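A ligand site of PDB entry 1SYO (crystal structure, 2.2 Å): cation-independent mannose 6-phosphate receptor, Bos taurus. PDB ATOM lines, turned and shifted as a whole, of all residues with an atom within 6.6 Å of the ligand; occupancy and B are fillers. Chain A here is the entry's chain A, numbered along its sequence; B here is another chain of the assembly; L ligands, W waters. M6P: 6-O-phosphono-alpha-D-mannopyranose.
Gln 356 of chain A touches the ligand.
CG of Lys 358 touches O2 of the ligand (3.9 Å).
Cys 385 touches the ligand (C to O2P, 3.4 Å).
Hydrophobic or aromatic side chains within 4 Å of the ligand: Tyr 324 of chain A and Tyr 421.
The nearest printed residue that does not touch the ligand is Ser 387 (4.8 Å).
The side-chain hydroxyl (OH) of Tyr 421 lies within hydrogen-bond range of the side-chain carboxylate (OE2) of Glu 416 (3.4 Å).
The side-chain carboxylate of Glu 416 lies within hydrogen-bond range of the backbone NH of Cys 419, at 3.4 Å.
The side-chain hydroxyl (OH) of Tyr 421 sits at hydrogen-bond distance from the guanidinium group (NE) of Arg 391 (2.9 Å).
The guanidinium group (NH2) of Arg 391 sits close to the side-chain sulfur (SG) of Cys 385.
The backbone NH (N) of Gln 348 sits at hydrogen-bond distance from the backbone carbonyl oxygen (O) of Lys 358, 2.6 Å away.
OH of Tyr 326 is in hydrogen-bond range of OE1 of Gln 348 (2.8 Å).
The side-chain sulfur of Cys 419 is disulfide-bonded to the side-chain sulfur of Cys 385 (2.0 Å).
N of Lys 350 of chain B is in hydrogen-bond range of O of Gln 356 of chain B (3.2 Å).
Water W1 lies within hydrogen-bond range of an oxygen (O5) of the ligand (2.9 Å), the side-chain amino group of Lys 350 of chain B (3.1 Å) and the guanidinium group of Arg 391 (3.1 Å).
Water W6 lies within hydrogen-bond range of the backbone NH of Ser 387 (2.6 Å), the side-chain hydroxyl of Ser 386 (2.6 Å) and an oxygen (O3P) of the ligand (3.3 Å).
Water W4 lies within hydrogen-bond range of the backbone NH of Ser 386, an oxygen (O2P) of the ligand and the backbone carbonyl oxygen of Glu 384.
Water W5 lies within hydrogen-bond range of the side-chain amino group (NZ) of Lys 350 of chain B (2.8 Å) and an oxygen (O5) of the ligand (3.5 Å).
The backbone NH (N) of Ser 386 is in hydrogen-bond range of an oxygen (O2P) of the ligand, at 2.5 Å.
An oxygen (O3P) of the ligand lies within hydrogen-bond range of the side-chain hydroxyl of Ser 386 (2.8 Å).
The side-chain carboxylate (OE2) of Glu 416 sits at hydrogen-bond distance from an oxygen (O4) of the ligand, at 2.6 Å.
OH of Tyr 421 sits at hydrogen-bond distance from O3 of the ligand (2.7 Å).
The guanidinium group (NE) of Arg 391 lies within hydrogen-bond range of an oxygen (O2) of the ligand, at 2.7 Å.
OH of Tyr 324 of chain A is in hydrogen-bond range of O1 of the ligand.
An oxygen (O2) of the ligand sits at hydrogen-bond distance from the side-chain amide nitrogen (NE2) of Gln 348, 3.0 Å away.
O4 of the ligand sits at hydrogen-bond distance from SG of Cys 419, 3.6 Å away.
An oxygen (O1P) of the ligand is in salt-bridge range of the side-chain amino group (NZ) of Lys 350 of chain B (3.8 Å).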
ATOM      1  N   LYS A 125       2.450 -21.378  22.332  1.00  0.00           N
ATOM      2  CA  LYS A 125       1.892 -21.036  23.627  1.00  0.00           C
ATOM      3  C   LYS A 125       1.799 -22.330  24.425  1.00  0.00           C
ATOM      4  O   LYS A 125       0.904 -23.150  24.223  1.00  0.00           O
ATOM      5  CB  LYS A 125       0.506 -20.416  23.446  1.00  0.00           C
ATOM      6  CG  LYS A 125       0.557 -19.061  22.761  1.00  0.00           C
ATOM      7  CD  LYS A 125      -0.847 -18.543  22.428  1.00  0.00           C
ATOM      8  CE  LYS A 125      -0.790 -17.126  21.862  1.00  0.00           C
ATOM      9  NZ  LYS A 125       0.144 -17.035  20.703  1.00  0.00           N
ATOM     10  N   TYR A 324     -19.109 -14.368  14.412  1.00  0.00           N
ATOM     11  CA  TYR A 324     -18.694 -14.896  13.107  1.00  0.00           C
ATOM     12  C   TYR A 324     -19.805 -15.686  12.443  1.00  0.00           C
ATOM     13  O   TYR A 324     -20.834 -15.997  13.052  1.00  0.00           O
ATOM     14  CB  TYR A 324     -17.471 -15.811  13.246  1.00  0.00           C
ATOM     15  CG  TYR A 324     -16.288 -15.217  13.956  1.00  0.00           C
ATOM     16  CD1 TYR A 324     -16.290 -15.073  15.352  1.00  0.00           C
ATOM     17  CD2 TYR A 324     -15.160 -14.803  13.253  1.00  0.00           C
ATOM     18  CE1 TYR A 324     -15.187 -14.533  16.027  1.00  0.00           C
ATOM     19  CE2 TYR A 324     -14.055 -14.262  13.913  1.00  0.00           C
ATOM     20  CZ  TYR A 324     -14.076 -14.131  15.299  1.00  0.00           C
ATOM     21  OH  TYR A 324     -12.979 -13.620  15.971  1.00  0.00           O
ATOM     22  N   TYR A 326     -20.252 -19.204  10.188  1.00  0.00           N
ATOM     23  CA  TYR A 326     -19.572 -20.424   9.770  1.00  0.00           C
ATOM     24  C   TYR A 326     -20.247 -21.036   8.560  1.00  0.00           C
ATOM     25  O   TYR A 326     -21.455 -21.259   8.566  1.00  0.00           O
ATOM     26  CB  TYR A 326     -19.516 -21.443  10.908  1.00  0.00           C
ATOM     27  CG  TYR A 326     -18.769 -20.956  12.140  1.00  0.00           C
ATOM     28  CD1 TYR A 326     -19.408 -20.174  13.097  1.00  0.00           C
ATOM     29  CD2 TYR A 326     -17.423 -21.248  12.338  1.00  0.00           C
ATOM     30  CE1 TYR A 326     -18.724 -19.688  14.214  1.00  0.00           C
ATOM     31  CE2 TYR A 326     -16.725 -20.779  13.448  1.00  0.00           C
ATOM     32  CZ  TYR A 326     -17.381 -19.990  14.382  1.00  0.00           C
ATOM     33  OH  TYR A 326     -16.720 -19.505  15.481  1.00  0.00           O
ATOM     34  N   GLN A 348     -14.594 -19.682   8.405  1.00  0.00           N
ATOM     35  CA  GLN A 348     -15.077 -18.696   9.369  1.00  0.00           C
ATOM     36  C   GLN A 348     -14.887 -17.266   8.885  1.00  0.00           C
ATOM     37  O   GLN A 348     -13.795 -16.867   8.484  1.00  0.00           O
ATOM     38  CB  GLN A 348     -14.356 -18.860  10.716  1.00  0.00           C
ATOM     39  CG  GLN A 348     -15.092 -18.219  11.895  1.00  0.00           C
ATOM     40  CD  GLN A 348     -14.198 -18.006  13.098  1.00  0.00           C
ATOM     41  OE1 GLN A 348     -14.623 -18.198  14.244  1.00  0.00           O
ATOM     42  NE2 GLN A 348     -12.961 -17.586  12.845  1.00  0.00           N
ATOM     43  N   LYS A 350     -15.436 -13.131   9.845  1.00  0.00           N
ATOM     44  CA  LYS A 350     -15.629 -12.161  10.931  1.00  0.00           C
ATOM     45  C   LYS A 350     -16.860 -11.299  10.616  1.00  0.00           C
ATOM     46  O   LYS A 350     -16.914 -10.674   9.559  1.00  0.00           O
ATOM     47  CB  LYS A 350     -14.390 -11.279  11.068  1.00  0.00           C
ATOM     48  CG  LYS A 350     -14.223 -10.603  12.416  1.00  0.00           C
ATOM     49  CD  LYS A 350     -12.911  -9.840  12.483  1.00  0.00           C
ATOM     50  CE  LYS A 350     -12.651  -9.343  13.895  1.00  0.00           C
ATOM     51  NZ  LYS A 350     -11.400  -8.543  13.971  1.00  0.00           N
ATOM     52  N   GLN A 356     -11.830 -10.718   7.152  1.00  0.00           N
ATOM     53  CA  GLN A 356     -11.099 -11.655   7.990  1.00  0.00           C
ATOM     54  C   GLN A 356     -11.800 -13.015   7.861  1.00  0.00           C
ATOM     55  O   GLN A 356     -12.876 -13.238   8.427  1.00  0.00           O
ATOM     56  CB  GLN A 356     -11.062 -11.184   9.450  1.00  0.00           C
ATOM     57  CG  GLN A 356     -10.108 -11.973  10.334  1.00  0.00           C
ATOM     58  CD  GLN A 356      -9.910 -11.338  11.712  1.00  0.00           C
ATOM     59  OE1 GLN A 356      -9.353 -10.257  11.831  1.00  0.00           O
ATOM     60  NE2 GLN A 356     -10.382 -12.023  12.746  1.00  0.00           N
ATOM     61  N   LYS A 358     -11.212 -17.339   7.930  1.00  0.00           N
ATOM     62  CA  LYS A 358     -10.321 -18.365   8.468  1.00  0.00           C
ATOM     63  C   LYS A 358     -10.811 -19.772   8.156  1.00  0.00           C
ATOM     64  O   LYS A 358     -11.994 -20.068   8.317  1.00  0.00           O
ATOM     65  CB  LYS A 358     -10.213 -18.201   9.987  1.00  0.00           C
ATOM     66  CG  LYS A 358      -9.744 -16.822  10.452  1.00  0.00           C
ATOM     67  CD  LYS A 358      -8.263 -16.602  10.160  1.00  0.00           C
ATOM     68  CE  LYS A 358      -7.764 -15.320  10.807  1.00  0.00           C
ATOM     69  NZ  LYS A 358      -6.280 -15.136  10.627  1.00  0.00           N
ATOM     70  N   GLU A 384      -3.498 -21.758  11.223  1.00  0.00           N
ATOM     71  CA  GLU A 384      -2.876 -21.694  12.538  1.00  0.00           C
ATOM     72  C   GLU A 384      -3.318 -20.526  13.412  1.00  0.00           C
ATOM     73  O   GLU A 384      -3.502 -19.416  12.929  1.00  0.00           O
ATOM     74  CB  GLU A 384      -1.353 -21.627  12.412  1.00  0.00           C
ATOM     75  CG  GLU A 384      -0.680 -22.874  11.863  1.00  0.00           C
ATOM     76  CD  GLU A 384       0.782 -22.973  12.304  1.00  0.00           C
ATOM     77  OE1 GLU A 384       1.455 -23.958  11.930  1.00  0.00           O
ATOM     78  OE2 GLU A 384       1.252 -22.075  13.049  1.00  0.00           O
ATOM     79  N   CYS A 385      -3.494 -20.796  14.700  1.00  0.00           N
ATOM     80  CA  CYS A 385      -3.838 -19.761  15.656  1.00  0.00           C
ATOM     81  C   CYS A 385      -2.499 -19.429  16.325  1.00  0.00           C
ATOM     82  O   CYS A 385      -1.617 -20.274  16.374  1.00  0.00           O
ATOM     83  CB  CYS A 385      -4.855 -20.294  16.680  1.00  0.00           C
ATOM     84  SG  CYS A 385      -6.568 -20.254  16.066  1.00  0.00           S
ATOM     85  N   SER A 386      -2.340 -18.213  16.824  1.00  0.00           N
ATOM     86  CA  SER A 386      -1.081 -17.808  17.459  1.00  0.00           C
ATOM     87  C   SER A 386      -0.393 -18.907  18.273  1.00  0.00           C
ATOM     88  O   SER A 386       0.827 -18.992  18.298  1.00  0.00           O
ATOM     89  CB  SER A 386      -1.299 -16.570  18.332  1.00  0.00           C
ATOM     90  OG  SER A 386      -2.214 -16.832  19.374  1.00  0.00           O
ATOM     91  N   SER A 387      -1.186 -19.749  18.947  1.00  0.00           N
ATOM     92  CA  SER A 387      -0.636 -20.843  19.744  1.00  0.00           C
ATOM     93  C   SER A 387       0.119 -21.807  18.831  1.00  0.00           C
ATOM     94  O   SER A 387       1.089 -22.450  19.242  1.00  0.00           O
ATOM     95  CB  SER A 387      -1.758 -21.598  20.452  1.00  0.00           C
ATOM     96  OG  SER A 387      -2.608 -22.260  19.517  1.00  0.00           O
ATOM     97  N   ARG A 391      -6.493 -24.699  13.122  1.00  0.00           N
ATOM     98  CA  ARG A 391      -7.915 -24.790  13.431  1.00  0.00           C
ATOM     99  C   ARG A 391      -8.509 -26.127  13.046  1.00  0.00           C
ATOM    100  O   ARG A 391      -8.059 -26.775  12.102  1.00  0.00           O
ATOM    101  CB  ARG A 391      -8.696 -23.646  12.772  1.00  0.00           C
ATOM    102  CG  ARG A 391      -8.506 -22.316  13.497  1.00  0.00           C
ATOM    103  CD  ARG A 391      -9.451 -21.263  12.961  1.00  0.00           C
ATOM    104  NE  ARG A 391      -9.088 -19.923  13.402  1.00  0.00           N
ATOM    105  CZ  ARG A 391      -7.918 -19.332  13.131  1.00  0.00           C
ATOM    106  NH1 ARG A 391      -6.998 -19.959  12.421  1.00  0.00           N
ATOM    107  NH2 ARG A 391      -7.689 -18.091  13.562  1.00  0.00           N
ATOM    108  N   GLU A 416     -16.807 -22.522  20.642  1.00  0.00           N
ATOM    109  CA  GLU A 416     -15.382 -22.651  20.319  1.00  0.00           C
ATOM    110  C   GLU A 416     -14.526 -22.825  21.562  1.00  0.00           C
ATOM    111  O   GLU A 416     -14.766 -22.176  22.569  1.00  0.00           O
ATOM    112  CB  GLU A 416     -14.873 -21.408  19.571  1.00  0.00           C
ATOM    113  CG  GLU A 416     -13.421 -21.056  19.921  1.00  0.00           C
ATOM    114  CD  GLU A 416     -12.828 -19.958  19.052  1.00  0.00           C
ATOM    115  OE1 GLU A 416     -13.545 -18.988  18.719  1.00  0.00           O
ATOM    116  OE2 GLU A 416     -11.627 -20.067  18.708  1.00  0.00           O
ATOM    117  N   ASP A 418     -10.453 -22.811  22.201  1.00  0.00           N
ATOM    118  CA  ASP A 418      -9.050 -22.709  21.791  1.00  0.00           C
ATOM    119  C   ASP A 418      -8.774 -23.261  20.387  1.00  0.00           C
ATOM    120  O   ASP A 418      -8.013 -24.213  20.199  1.00  0.00           O
ATOM    121  CB  ASP A 418      -8.142 -23.405  22.804  1.00  0.00           C
ATOM    122  CG  ASP A 418      -8.213 -22.760  24.183  1.00  0.00           C
ATOM    123  OD1 ASP A 418      -8.133 -21.516  24.273  1.00  0.00           O
ATOM    124  OD2 ASP A 418      -8.338 -23.506  25.173  1.00  0.00           O
ATOM    125  N   CYS A 419      -9.432 -22.614  19.431  1.00  0.00           N
ATOM    126  CA  CYS A 419      -9.351 -22.897  18.014  1.00  0.00           C
ATOM    127  C   CYS A 419      -9.864 -24.240  17.489  1.00  0.00           C
ATOM    128  O   CYS A 419      -9.436 -24.714  16.433  1.00  0.00           O
ATOM    129  CB  CYS A 419      -7.935 -22.581  17.527  1.00  0.00           C
ATOM    130  SG  CYS A 419      -7.687 -20.776  17.664  1.00  0.00           S
ATOM    131  N   TYR A 421     -13.650 -25.740  16.770  1.00  0.00           N
ATOM    132  CA  TYR A 421     -15.036 -25.303  16.727  1.00  0.00           C
ATOM    133  C   TYR A 421     -16.025 -26.464  16.717  1.00  0.00           C
ATOM    134  O   TYR A 421     -15.926 -27.380  15.895  1.00  0.00           O
ATOM    135  CB  TYR A 421     -15.238 -24.391  15.513  1.00  0.00           C
ATOM    136  CG  TYR A 421     -14.178 -23.301  15.420  1.00  0.00           C
ATOM    137  CD1 TYR A 421     -12.867 -23.611  15.047  1.00  0.00           C
ATOM    138  CD2 TYR A 421     -14.464 -21.981  15.753  1.00  0.00           C
ATOM    139  CE1 TYR A 421     -11.873 -22.633  15.016  1.00  0.00           C
ATOM    140  CE2 TYR A 421     -13.475 -20.991  15.729  1.00  0.00           C
ATOM    141  CZ  TYR A 421     -12.176 -21.320  15.361  1.00  0.00           C
ATOM    142  OH  TYR A 421     -11.175 -20.365  15.344  1.00  0.00           O
ATOM    143  N   GLU B 323       4.181  -9.051  17.539  1.00  0.00           N
ATOM    144  CA  GLU B 323       3.295  -9.866  16.710  1.00  0.00           C
ATOM    145  C   GLU B 323       3.073  -9.342  15.302  1.00  0.00           C
ATOM    146  O   GLU B 323       2.540 -10.057  14.453  1.00  0.00           O
ATOM    147  CB  GLU B 323       1.932 -10.001  17.394  1.00  0.00           C
ATOM    148  CG  GLU B 323       1.970 -10.668  18.740  1.00  0.00           C
ATOM    149  CD  GLU B 323       0.627 -10.623  19.433  1.00  0.00           C
ATOM    150  OE1 GLU B 323      -0.353 -11.177  18.887  1.00  0.00           O
ATOM    151  OE2 GLU B 323       0.553 -10.019  20.537  1.00  0.00           O
ATOM    152  N   TYR B 324       3.466  -8.106  15.031  1.00  0.00           N
ATOM    153  CA  TYR B 324       3.267  -7.575  13.699  1.00  0.00           C
ATOM    154  C   TYR B 324       4.472  -6.832  13.171  1.00  0.00           C
ATOM    155  O   TYR B 324       5.454  -6.625  13.878  1.00  0.00           O
ATOM    156  CB  TYR B 324       2.070  -6.607  13.653  1.00  0.00           C
ATOM    157  CG  TYR B 324       0.764  -7.178  14.136  1.00  0.00           C
ATOM    158  CD1 TYR B 324       0.492  -7.289  15.501  1.00  0.00           C
ATOM    159  CD2 TYR B 324      -0.221  -7.582  13.236  1.00  0.00           C
ATOM    160  CE1 TYR B 324      -0.727  -7.784  15.951  1.00  0.00           C
ATOM    161  CE2 TYR B 324      -1.442  -8.082  13.679  1.00  0.00           C
ATOM    162  CZ  TYR B 324      -1.685  -8.186  15.041  1.00  0.00           C
ATOM    163  OH  TYR B 324      -2.887  -8.675  15.493  1.00  0.00           O
ATOM    164  N   LYS B 350       0.536  -9.411  10.234  1.00  0.00           N
ATOM    165  CA  LYS B 350       0.622 -10.390  11.321  1.00  0.00           C
ATOM    166  C   LYS B 350       1.803 -11.315  11.039  1.00  0.00           C
ATOM    167  O   LYS B 350       1.935 -11.812   9.928  1.00  0.00           O
ATOM    168  CB  LYS B 350      -0.676 -11.207  11.388  1.00  0.00           C
ATOM    169  CG  LYS B 350      -0.970 -11.834  12.736  1.00  0.00           C
ATOM    170  CD  LYS B 350      -2.345 -12.443  12.764  1.00  0.00           C
ATOM    171  CE  LYS B 350      -2.786 -12.752  14.186  1.00  0.00           C
ATOM    172  NZ  LYS B 350      -4.210 -13.188  14.278  1.00  0.00           N
ATOM    173  N   GLN B 356      -2.607 -11.929   6.869  1.00  0.00           N
ATOM    174  CA  GLN B 356      -3.484 -11.059   7.637  1.00  0.00           C
ATOM    175  C   GLN B 356      -2.911  -9.652   7.538  1.00  0.00           C
ATOM    176  O   GLN B 356      -1.952  -9.294   8.238  1.00  0.00           O
ATOM    177  CB  GLN B 356      -3.572 -11.481   9.112  1.00  0.00           C
ATOM    178  CG  GLN B 356      -4.652 -10.704   9.890  1.00  0.00           C
ATOM    179  CD  GLN B 356      -4.963 -11.298  11.259  1.00  0.00           C
ATOM    180  OE1 GLN B 356      -5.324 -12.470  11.373  1.00  0.00           O
ATOM    181  NE2 GLN B 356      -4.843 -10.477  12.297  1.00  0.00           N
HETATM  182  C1  M6P L   1      -9.790 -15.469  14.957  1.00  0.00           C
HETATM  183  C2  M6P L   1     -10.848 -16.602  14.990  1.00  0.00           C
HETATM  184  C3  M6P L   1     -11.116 -17.079  16.466  1.00  0.00           C
HETATM  185  C4  M6P L   1      -9.789 -17.588  17.061  1.00  0.00           C
HETATM  186  C5  M6P L   1      -8.783 -16.403  17.061  1.00  0.00           C
HETATM  187  C6  M6P L   1      -7.424 -16.779  17.590  1.00  0.00           C
HETATM  188  O1  M6P L   1     -10.302 -14.304  15.643  1.00  0.00           O
HETATM  189  O2  M6P L   1     -10.285 -17.692  14.259  1.00  0.00           O
HETATM  190  O3  M6P L   1     -12.086 -18.118  16.468  1.00  0.00           O
HETATM  191  O4  M6P L   1      -9.982 -18.042  18.406  1.00  0.00           O
HETATM  192  O5  M6P L   1      -8.584 -15.911  15.662  1.00  0.00           O
HETATM  193  O6  M6P L   1      -6.605 -15.625  17.577  1.00  0.00           O
HETATM  194  P   M6P L   1      -5.109 -15.702  18.067  1.00  0.00           P
HETATM  195  O1P M6P L   1      -4.427 -14.237  17.965  1.00  0.00           O
HETATM  196  O2P M6P L   1      -4.346 -16.671  17.041  1.00  0.00           O
HETATM  197  O3P M6P L   1      -5.001 -16.300  19.555  1.00  0.00           O
HETATM  198  O   HOH W   1      -5.879 -15.730  14.577  1.00  0.00           O
HETATM  199  O   HOH W   2      -6.412 -11.447  17.328  1.00  0.00           O
HETATM  200  O   HOH W   3      -6.423 -16.224  21.812  1.00  0.00           O
HETATM  201  O   HOH W   4      -2.411 -16.423  14.287  1.00  0.00           O
HETATM  202  O   HOH W   5      -6.883 -12.908  15.135  1.00  0.00           O
HETATM  203  O   HOH W   6      -3.378 -19.091  20.094  1.00  0.00           O
